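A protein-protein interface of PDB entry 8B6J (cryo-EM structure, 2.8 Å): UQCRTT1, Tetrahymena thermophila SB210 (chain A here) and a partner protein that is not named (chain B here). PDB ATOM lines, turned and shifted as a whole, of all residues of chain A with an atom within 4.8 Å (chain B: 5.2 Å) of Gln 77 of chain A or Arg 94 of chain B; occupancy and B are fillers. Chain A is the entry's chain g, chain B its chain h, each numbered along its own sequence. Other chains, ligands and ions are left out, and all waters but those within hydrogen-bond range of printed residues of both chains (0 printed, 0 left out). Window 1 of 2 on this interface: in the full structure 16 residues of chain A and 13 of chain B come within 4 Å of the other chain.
Of the 11 printed residues of chain B, 4 touch a printed residue of chain A.
Printed residues of chain B that touch a printed residue of chain A: Gln 90, Arg 94, Arg 95 and Arg 98.
Hydrophobic or aromatic side chains of chain A that line the printed part of chain B: Ile 74 and Tyr 133.
Of the printed residues of chain B, Asp 73 of chain A touches Arg 94.
Printed residues of chain B within 4 Å of Arg 78 of chain A: Arg 95.
Phe 132 of chain A touches none of the printed residues of chain B.
Of the printed residues of chain B, Tyr 133 of chain A touches Gln 90 and Arg 94.
Of chain A, only Asp 73, Gln 77 and Tyr 133 come within 4 Å of Arg 94 of chain B.
Printed residues of chain A within 4 Å of Arg 95 of chain B: Arg 78.
Asn 96 of chain B touches none of the printed residues of chain A.
Of the printed residues of chain A, Arg 98 of chain B touches Ile 74 (3.9 Å).
The nearest printed residue of chain A that does not touch Arg 98 of chain B is Asp 73 of chain A (4.8 Å).
Among the printed residues, pairs that only touch across the chains: Ile 74 of chain A with Arg 98 of chain B and Tyr 133 of chain A with Gln 90 of chain B.
The guanidinium group of Arg 94 of chain B is in salt-bridge range of the side-chain carboxylate of Asp 73 of chain A (3.3 Å).
OE1 of Gln 77 of chain A sits at hydrogen-bond distance from NE of Arg 94 of chain B (2.9 Å).
The side-chain hydroxyl of Tyr 133 of chain A is in hydrogen-bond range of the guanidinium group of Arg 94 of chain B.
NH2 of Arg 95 of chain B sits close to NH2 of Arg 78 of chain A (3.3 Å).
The guanidinium group (NH2) of Arg 139 of chain A lies within salt-bridge range of the side-chain carboxylate (OD1) of Asp 73 of chain A.
The backbone carbonyl oxygen of Gln 77 of chain A lies within hydrogen-bond range of the backbone NH of Val 134 of chain A (3.1 Å).
The backbone carbonyl oxygen of Lys 89 of chain B lies within hydrogen-bond range of the backbone NH of Arg 94 of chain B.
The backbone carbonyl oxygen (O) of Tyr 93 of chain B lies within hydrogen-bond range of the backbone NH (N) of Arg 98 of chain B (2.7 Å).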
ATOM      1  N   ASP A  73       4.103 -10.762 -23.464  1.00  0.00           N
ATOM      2  CA  ASP A  73       4.726 -12.055 -23.711  1.00  0.00           C
ATOM      3  C   ASP A  73       6.210 -12.018 -23.379  1.00  0.00           C
ATOM      4  O   ASP A  73       6.735 -12.945 -22.751  1.00  0.00           O
ATOM      5  CB  ASP A  73       4.513 -12.468 -25.167  1.00  0.00           C
ATOM      6  CG  ASP A  73       4.996 -13.876 -25.450  1.00  0.00           C
ATOM      7  OD1 ASP A  73       5.353 -14.589 -24.489  1.00  0.00           O
ATOM      8  OD2 ASP A  73       5.021 -14.272 -26.634  1.00  0.00           O
ATOM      9  N   ILE A  74       6.904 -10.952 -23.782  1.00  0.00           N
ATOM     10  CA  ILE A  74       8.332 -10.855 -23.479  1.00  0.00           C
ATOM     11  C   ILE A  74       8.551 -10.794 -21.971  1.00  0.00           C
ATOM     12  O   ILE A  74       9.413 -11.493 -21.417  1.00  0.00           O
ATOM     13  CB  ILE A  74       8.950  -9.641 -24.195  1.00  0.00           C
ATOM     14  CG1 ILE A  74       9.004  -9.903 -25.703  1.00  0.00           C
ATOM     15  CG2 ILE A  74      10.338  -9.350 -23.645  1.00  0.00           C
ATOM     16  CD1 ILE A  74       9.347  -8.689 -26.533  1.00  0.00           C
ATOM     17  N   ALA A  75       7.761  -9.971 -21.279  1.00  0.00           N
ATOM     18  CA  ALA A  75       7.914  -9.844 -19.834  1.00  0.00           C
ATOM     19  C   ALA A  75       7.659 -11.172 -19.133  1.00  0.00           C
ATOM     20  O   ALA A  75       8.404 -11.555 -18.225  1.00  0.00           O
ATOM     21  CB  ALA A  75       6.967  -8.769 -19.302  1.00  0.00           C
ATOM     22  N   HIS A  76       6.614 -11.892 -19.544  1.00  0.00           N
ATOM     23  CA  HIS A  76       6.332 -13.187 -18.939  1.00  0.00           C
ATOM     24  C   HIS A  76       7.452 -14.178 -19.220  1.00  0.00           C
ATOM     25  O   HIS A  76       7.820 -14.973 -18.349  1.00  0.00           O
ATOM     26  CB  HIS A  76       4.995 -13.723 -19.448  1.00  0.00           C
ATOM     27  CG  HIS A  76       3.805 -13.078 -18.807  1.00  0.00           C
ATOM     28  ND1 HIS A  76       3.910 -12.225 -17.730  1.00  0.00           N
ATOM     29  CD2 HIS A  76       2.484 -13.165 -19.089  1.00  0.00           C
ATOM     30  CE1 HIS A  76       2.707 -11.813 -17.377  1.00  0.00           C
ATOM     31  NE2 HIS A  76       1.823 -12.369 -18.186  1.00  0.00           N
ATOM     32  N   GLN A  77       8.007 -14.150 -20.434  1.00  0.00           N
ATOM     33  CA  GLN A  77       9.181 -14.966 -20.717  1.00  0.00           C
ATOM     34  C   GLN A  77      10.303 -14.650 -19.742  1.00  0.00           C
ATOM     35  O   GLN A  77      11.042 -15.546 -19.320  1.00  0.00           O
ATOM     36  CB  GLN A  77       9.650 -14.739 -22.154  1.00  0.00           C
ATOM     37  CG  GLN A  77      10.926 -15.486 -22.523  1.00  0.00           C
ATOM     38  CD  GLN A  77      11.556 -14.967 -23.795  1.00  0.00           C
ATOM     39  OE1 GLN A  77      10.980 -14.133 -24.493  1.00  0.00           O
ATOM     40  NE2 GLN A  77      12.752 -15.454 -24.103  1.00  0.00           N
ATOM     41  N   ARG A  78      10.447 -13.380 -19.375  1.00  0.00           N
ATOM     42  CA  ARG A  78      11.487 -12.961 -18.446  1.00  0.00           C
ATOM     43  C   ARG A  78      11.050 -13.034 -16.989  1.00  0.00           C
ATOM     44  O   ARG A  78      11.816 -12.632 -16.110  1.00  0.00           O
ATOM     45  CB  ARG A  78      11.938 -11.537 -18.775  1.00  0.00           C
ATOM     46  CG  ARG A  78      12.592 -11.412 -20.134  1.00  0.00           C
ATOM     47  CD  ARG A  78      12.844  -9.966 -20.500  1.00  0.00           C
ATOM     48  NE  ARG A  78      13.488  -9.843 -21.801  1.00  0.00           N
ATOM     49  CZ  ARG A  78      13.723  -8.692 -22.415  1.00  0.00           C
ATOM     50  NH1 ARG A  78      13.369  -7.536 -21.876  1.00  0.00           N
ATOM     51  NH2 ARG A  78      14.326  -8.701 -23.599  1.00  0.00           N
ATOM     52  N   GLY A  79       9.853 -13.544 -16.710  1.00  0.00           N
ATOM     53  CA  GLY A  79       9.372 -13.594 -15.345  1.00  0.00           C
ATOM     54  C   GLY A  79       8.967 -12.253 -14.787  1.00  0.00           C
ATOM     55  O   GLY A  79       8.937 -12.080 -13.567  1.00  0.00           O
ATOM     56  N   TYR A 122      16.459 -13.271 -13.627  1.00  0.00           N
ATOM     57  CA  TYR A 122      16.518 -13.745 -15.002  1.00  0.00           C
ATOM     58  C   TYR A 122      17.917 -13.596 -15.582  1.00  0.00           C
ATOM     59  O   TYR A 122      18.398 -14.488 -16.289  1.00  0.00           O
ATOM     60  CB  TYR A 122      15.503 -12.987 -15.857  1.00  0.00           C
ATOM     61  CG  TYR A 122      15.497 -13.399 -17.310  1.00  0.00           C
ATOM     62  CD1 TYR A 122      14.775 -14.505 -17.733  1.00  0.00           C
ATOM     63  CD2 TYR A 122      16.205 -12.680 -18.259  1.00  0.00           C
ATOM     64  CE1 TYR A 122      14.765 -14.885 -19.059  1.00  0.00           C
ATOM     65  CE2 TYR A 122      16.200 -13.051 -19.586  1.00  0.00           C
ATOM     66  CZ  TYR A 122      15.478 -14.154 -19.981  1.00  0.00           C
ATOM     67  OH  TYR A 122      15.469 -14.529 -21.304  1.00  0.00           O
ATOM     68  N   PHE A 132      17.214 -18.271 -21.985  1.00  0.00           N
ATOM     69  CA  PHE A 132      16.521 -18.709 -20.782  1.00  0.00           C
ATOM     70  C   PHE A 132      15.035 -18.390 -20.868  1.00  0.00           C
ATOM     71  O   PHE A 132      14.643 -17.248 -21.128  1.00  0.00           O
ATOM     72  CB  PHE A 132      17.140 -18.041 -19.555  1.00  0.00           C
ATOM     73  CG  PHE A 132      16.514 -18.456 -18.254  1.00  0.00           C
ATOM     74  CD1 PHE A 132      16.313 -19.792 -17.958  1.00  0.00           C
ATOM     75  CD2 PHE A 132      16.146 -17.507 -17.318  1.00  0.00           C
ATOM     76  CE1 PHE A 132      15.743 -20.171 -16.762  1.00  0.00           C
ATOM     77  CE2 PHE A 132      15.579 -17.883 -16.119  1.00  0.00           C
ATOM     78  CZ  PHE A 132      15.378 -19.217 -15.841  1.00  0.00           C
ATOM     79  N   TYR A 133      14.209 -19.408 -20.647  1.00  0.00           N
ATOM     80  CA  TYR A 133      12.763 -19.261 -20.534  1.00  0.00           C
ATOM     81  C   TYR A 133      12.384 -19.481 -19.078  1.00  0.00           C
ATOM     82  O   TYR A 133      12.687 -20.534 -18.506  1.00  0.00           O
ATOM     83  CB  TYR A 133      12.034 -20.254 -21.438  1.00  0.00           C
ATOM     84  CG  TYR A 133      11.494 -19.647 -22.712  1.00  0.00           C
ATOM     85  CD1 TYR A 133      12.300 -19.502 -23.831  1.00  0.00           C
ATOM     86  CD2 TYR A 133      10.175 -19.227 -22.796  1.00  0.00           C
ATOM     87  CE1 TYR A 133      11.810 -18.950 -24.997  1.00  0.00           C
ATOM     88  CE2 TYR A 133       9.675 -18.676 -23.958  1.00  0.00           C
ATOM     89  CZ  TYR A 133      10.496 -18.540 -25.054  1.00  0.00           C
ATOM     90  OH  TYR A 133      10.001 -17.990 -26.212  1.00  0.00           O
ATOM     91  N   VAL A 134      11.725 -18.494 -18.485  1.00  0.00           N
ATOM     92  CA  VAL A 134      11.433 -18.563 -17.050  1.00  0.00           C
ATOM     93  C   VAL A 134      10.492 -19.732 -16.779  1.00  0.00           C
ATOM     94  O   VAL A 134       9.489 -19.898 -17.500  1.00  0.00           O
ATOM     95  CB  VAL A 134      10.826 -17.238 -16.566  1.00  0.00           C
ATOM     96  CG1 VAL A 134      10.053 -17.437 -15.286  1.00  0.00           C
ATOM     97  CG2 VAL A 134      11.924 -16.209 -16.363  1.00  0.00           C
ATOM     98  N   ARG A 139       6.674 -17.672 -13.587  1.00  0.00           N
ATOM     99  CA  ARG A 139       5.713 -17.068 -14.501  1.00  0.00           C
ATOM    100  C   ARG A 139       4.355 -16.899 -13.838  1.00  0.00           C
ATOM    101  O   ARG A 139       3.627 -15.954 -14.152  1.00  0.00           O
ATOM    102  CB  ARG A 139       5.590 -17.930 -15.758  1.00  0.00           C
ATOM    103  CG  ARG A 139       4.964 -17.233 -16.949  1.00  0.00           C
ATOM    104  CD  ARG A 139       4.695 -18.227 -18.069  1.00  0.00           C
ATOM    105  NE  ARG A 139       4.282 -17.577 -19.307  1.00  0.00           N
ATOM    106  CZ  ARG A 139       5.099 -17.254 -20.301  1.00  0.00           C
ATOM    107  NH1 ARG A 139       6.398 -17.500 -20.241  1.00  0.00           N
ATOM    108  NH2 ARG A 139       4.600 -16.670 -21.387  1.00  0.00           N
ATOM    109  N   PHE B  88      19.082 -21.876 -31.364  1.00  0.00           N
ATOM    110  CA  PHE B  88      18.508 -21.444 -32.632  1.00  0.00           C
ATOM    111  C   PHE B  88      17.089 -20.915 -32.493  1.00  0.00           C
ATOM    112  O   PHE B  88      16.792 -19.819 -32.975  1.00  0.00           O
ATOM    113  CB  PHE B  88      18.544 -22.607 -33.636  1.00  0.00           C
ATOM    114  CG  PHE B  88      19.907 -22.856 -34.230  1.00  0.00           C
ATOM    115  CD1 PHE B  88      20.651 -21.816 -34.761  1.00  0.00           C
ATOM    116  CD2 PHE B  88      20.444 -24.132 -34.251  1.00  0.00           C
ATOM    117  CE1 PHE B  88      21.900 -22.044 -35.303  1.00  0.00           C
ATOM    118  CE2 PHE B  88      21.693 -24.364 -34.791  1.00  0.00           C
ATOM    119  CZ  PHE B  88      22.422 -23.319 -35.317  1.00  0.00           C
ATOM    120  N   LYS B  89      16.195 -21.666 -31.848  1.00  0.00           N
ATOM    121  CA  LYS B  89      14.824 -21.193 -31.688  1.00  0.00           C
ATOM    122  C   LYS B  89      14.710 -20.137 -30.596  1.00  0.00           C
ATOM    123  O   LYS B  89      13.926 -19.191 -30.726  1.00  0.00           O
ATOM    124  CB  LYS B  89      13.893 -22.367 -31.387  1.00  0.00           C
ATOM    125  CG  LYS B  89      13.678 -23.300 -32.568  1.00  0.00           C
ATOM    126  CD  LYS B  89      12.708 -24.424 -32.236  1.00  0.00           C
ATOM    127  CE  LYS B  89      11.291 -23.909 -32.033  1.00  0.00           C
ATOM    128  NZ  LYS B  89      10.315 -25.020 -31.847  1.00  0.00           N
ATOM    129  N   GLN B  90      15.480 -20.276 -29.515  1.00  0.00           N
ATOM    130  CA  GLN B  90      15.347 -19.392 -28.364  1.00  0.00           C
ATOM    131  C   GLN B  90      16.394 -18.289 -28.313  1.00  0.00           C
ATOM    132  O   GLN B  90      16.183 -17.295 -27.610  1.00  0.00           O
ATOM    133  CB  GLN B  90      15.424 -20.204 -27.065  1.00  0.00           C
ATOM    134  CG  GLN B  90      14.313 -21.223 -26.903  1.00  0.00           C
ATOM    135  CD  GLN B  90      14.509 -22.110 -25.692  1.00  0.00           C
ATOM    136  OE1 GLN B  90      15.299 -21.801 -24.803  1.00  0.00           O
ATOM    137  NE2 GLN B  90      13.793 -23.226 -25.656  1.00  0.00           N
ATOM    138  N   VAL B  91      17.509 -18.433 -29.026  1.00  0.00           N
ATOM    139  CA  VAL B  91      18.581 -17.452 -29.009  1.00  0.00           C
ATOM    140  C   VAL B  91      18.677 -16.695 -30.329  1.00  0.00           C
ATOM    141  O   VAL B  91      18.854 -15.476 -30.334  1.00  0.00           O
ATOM    142  CB  VAL B  91      19.929 -18.118 -28.659  1.00  0.00           C
ATOM    143  CG1 VAL B  91      21.072 -17.134 -28.844  1.00  0.00           C
ATOM    144  CG2 VAL B  91      19.907 -18.644 -27.233  1.00  0.00           C
ATOM    145  N   TRP B  92      18.573 -17.395 -31.458  1.00  0.00           N
ATOM    146  CA  TRP B  92      18.663 -16.734 -32.754  1.00  0.00           C
ATOM    147  C   TRP B  92      17.315 -16.222 -33.244  1.00  0.00           C
ATOM    148  O   TRP B  92      17.228 -15.091 -33.730  1.00  0.00           O
ATOM    149  CB  TRP B  92      19.260 -17.683 -33.796  1.00  0.00           C
ATOM    150  CG  TRP B  92      20.756 -17.678 -33.821  1.00  0.00           C
ATOM    151  CD1 TRP B  92      21.593 -17.343 -32.798  1.00  0.00           C
ATOM    152  CD2 TRP B  92      21.595 -18.010 -34.933  1.00  0.00           C
ATOM    153  NE1 TRP B  92      22.901 -17.452 -33.202  1.00  0.00           N
ATOM    154  CE2 TRP B  92      22.929 -17.860 -34.509  1.00  0.00           C
ATOM    155  CE3 TRP B  92      21.347 -18.423 -36.245  1.00  0.00           C
ATOM    156  CZ2 TRP B  92      24.011 -18.107 -35.348  1.00  0.00           C
ATOM    157  CZ3 TRP B  92      22.422 -18.669 -37.078  1.00  0.00           C
ATOM    158  CH2 TRP B  92      23.738 -18.509 -36.626  1.00  0.00           C
ATOM    159  N   TYR B  93      16.258 -17.026 -33.131  1.00  0.00           N
ATOM    160  CA  TYR B  93      14.950 -16.581 -33.597  1.00  0.00           C
ATOM    161  C   TYR B  93      14.243 -15.737 -32.544  1.00  0.00           C
ATOM    162  O   TYR B  93      13.876 -14.585 -32.798  1.00  0.00           O
ATOM    163  CB  TYR B  93      14.081 -17.779 -33.983  1.00  0.00           C
ATOM    164  CG  TYR B  93      12.682 -17.380 -34.386  1.00  0.00           C
ATOM    165  CD1 TYR B  93      12.419 -16.901 -35.661  1.00  0.00           C
ATOM    166  CD2 TYR B  93      11.628 -17.467 -33.488  1.00  0.00           C
ATOM    167  CE1 TYR B  93      11.145 -16.528 -36.033  1.00  0.00           C
ATOM    168  CE2 TYR B  93      10.350 -17.096 -33.852  1.00  0.00           C
ATOM    169  CZ  TYR B  93      10.115 -16.626 -35.126  1.00  0.00           C
ATOM    170  OH  TYR B  93       8.844 -16.255 -35.495  1.00  0.00           O
ATOM    171  N   ARG B  94      14.048 -16.298 -31.349  1.00  0.00           N
ATOM    172  CA  ARG B  94      13.290 -15.599 -30.318  1.00  0.00           C
ATOM    173  C   ARG B  94      13.868 -14.223 -30.029  1.00  0.00           C
ATOM    174  O   ARG B  94      13.121 -13.291 -29.708  1.00  0.00           O
ATOM    175  CB  ARG B  94      13.258 -16.440 -29.041  1.00  0.00           C
ATOM    176  CG  ARG B  94      12.464 -15.827 -27.896  1.00  0.00           C
ATOM    177  CD  ARG B  94      10.984 -15.752 -28.215  1.00  0.00           C
ATOM    178  NE  ARG B  94      10.220 -15.170 -27.119  1.00  0.00           N
ATOM    179  CZ  ARG B  94       8.900 -15.054 -27.104  1.00  0.00           C
ATOM    180  NH1 ARG B  94       8.157 -15.485 -28.110  1.00  0.00           N
ATOM    181  NH2 ARG B  94       8.310 -14.494 -26.053  1.00  0.00           N
ATOM    182  N   ARG B  95      15.186 -14.069 -30.141  1.00  0.00           N
ATOM    183  CA  ARG B  95      15.861 -12.833 -29.769  1.00  0.00           C
ATOM    184  C   ARG B  95      16.220 -11.954 -30.959  1.00  0.00           C
ATOM    185  O   ARG B  95      16.086 -10.730 -30.870  1.00  0.00           O
ATOM    186  CB  ARG B  95      17.131 -13.152 -28.977  1.00  0.00           C
ATOM    187  CG  ARG B  95      16.962 -13.073 -27.471  1.00  0.00           C
ATOM    188  CD  ARG B  95      16.889 -11.632 -26.996  1.00  0.00           C
ATOM    189  NE  ARG B  95      16.959 -11.532 -25.543  1.00  0.00           N
ATOM    190  CZ  ARG B  95      17.087 -10.395 -24.874  1.00  0.00           C
ATOM    191  NH1 ARG B  95      17.167  -9.231 -25.497  1.00  0.00           N
ATOM    192  NH2 ARG B  95      17.139 -10.426 -23.546  1.00  0.00           N
ATOM    193  N   ASN B  96      16.667 -12.535 -32.072  1.00  0.00           N
ATOM    194  CA  ASN B  96      17.187 -11.750 -33.185  1.00  0.00           C
ATOM    195  C   ASN B  96      16.282 -11.788 -34.410  1.00  0.00           C
ATOM    196  O   ASN B  96      15.799 -10.741 -34.845  1.00  0.00           O
ATOM    197  CB  ASN B  96      18.592 -12.245 -33.554  1.00  0.00           C
ATOM    198  CG  ASN B  96      19.509 -12.343 -32.355  1.00  0.00           C
ATOM    199  OD1 ASN B  96      20.169 -13.359 -32.142  1.00  0.00           O
ATOM    200  ND2 ASN B  96      19.550 -11.284 -31.556  1.00  0.00           N
ATOM    201  N   ARG B  98      13.228 -12.984 -34.906  1.00  0.00           N
ATOM    202  CA  ARG B  98      11.840 -12.616 -34.658  1.00  0.00           C
ATOM    203  C   ARG B  98      11.647 -11.107 -34.647  1.00  0.00           C
ATOM    204  O   ARG B  98      10.521 -10.634 -34.836  1.00  0.00           O
ATOM    205  CB  ARG B  98      11.370 -13.215 -33.332  1.00  0.00           C
ATOM    206  CG  ARG B  98       9.869 -13.134 -33.105  1.00  0.00           C
ATOM    207  CD  ARG B  98       9.449 -13.944 -31.887  1.00  0.00           C
ATOM    208  NE  ARG B  98       9.424 -13.146 -30.667  1.00  0.00           N
ATOM    209  CZ  ARG B  98       8.333 -12.607 -30.136  1.00  0.00           C
ATOM    210  NH1 ARG B  98       7.142 -12.762 -30.689  1.00  0.00           N
ATOM    211  NH2 ARG B  98       8.441 -11.898 -29.018  1.00  0.00           N
ATOM    212  N   THR B  99      12.717 -10.342 -34.432  1.00  0.00           N
ATOM    213  CA  THR B  99      12.623  -8.890 -34.369  1.00  0.00           C
ATOM    214  C   THR B  99      12.803  -8.218 -35.724  1.00  0.00           C
ATOM    215  O   THR B  99      12.170  -7.186 -35.976  1.00  0.00           O
ATOM    216  CB  THR B  99      13.666  -8.337 -33.395  1.00  0.00           C
ATOM    217  OG1 THR B  99      14.981  -8.687 -33.844  1.00  0.00           O
ATOM    218  CG2 THR B  99      13.446  -8.898 -31.999  1.00  0.00           C
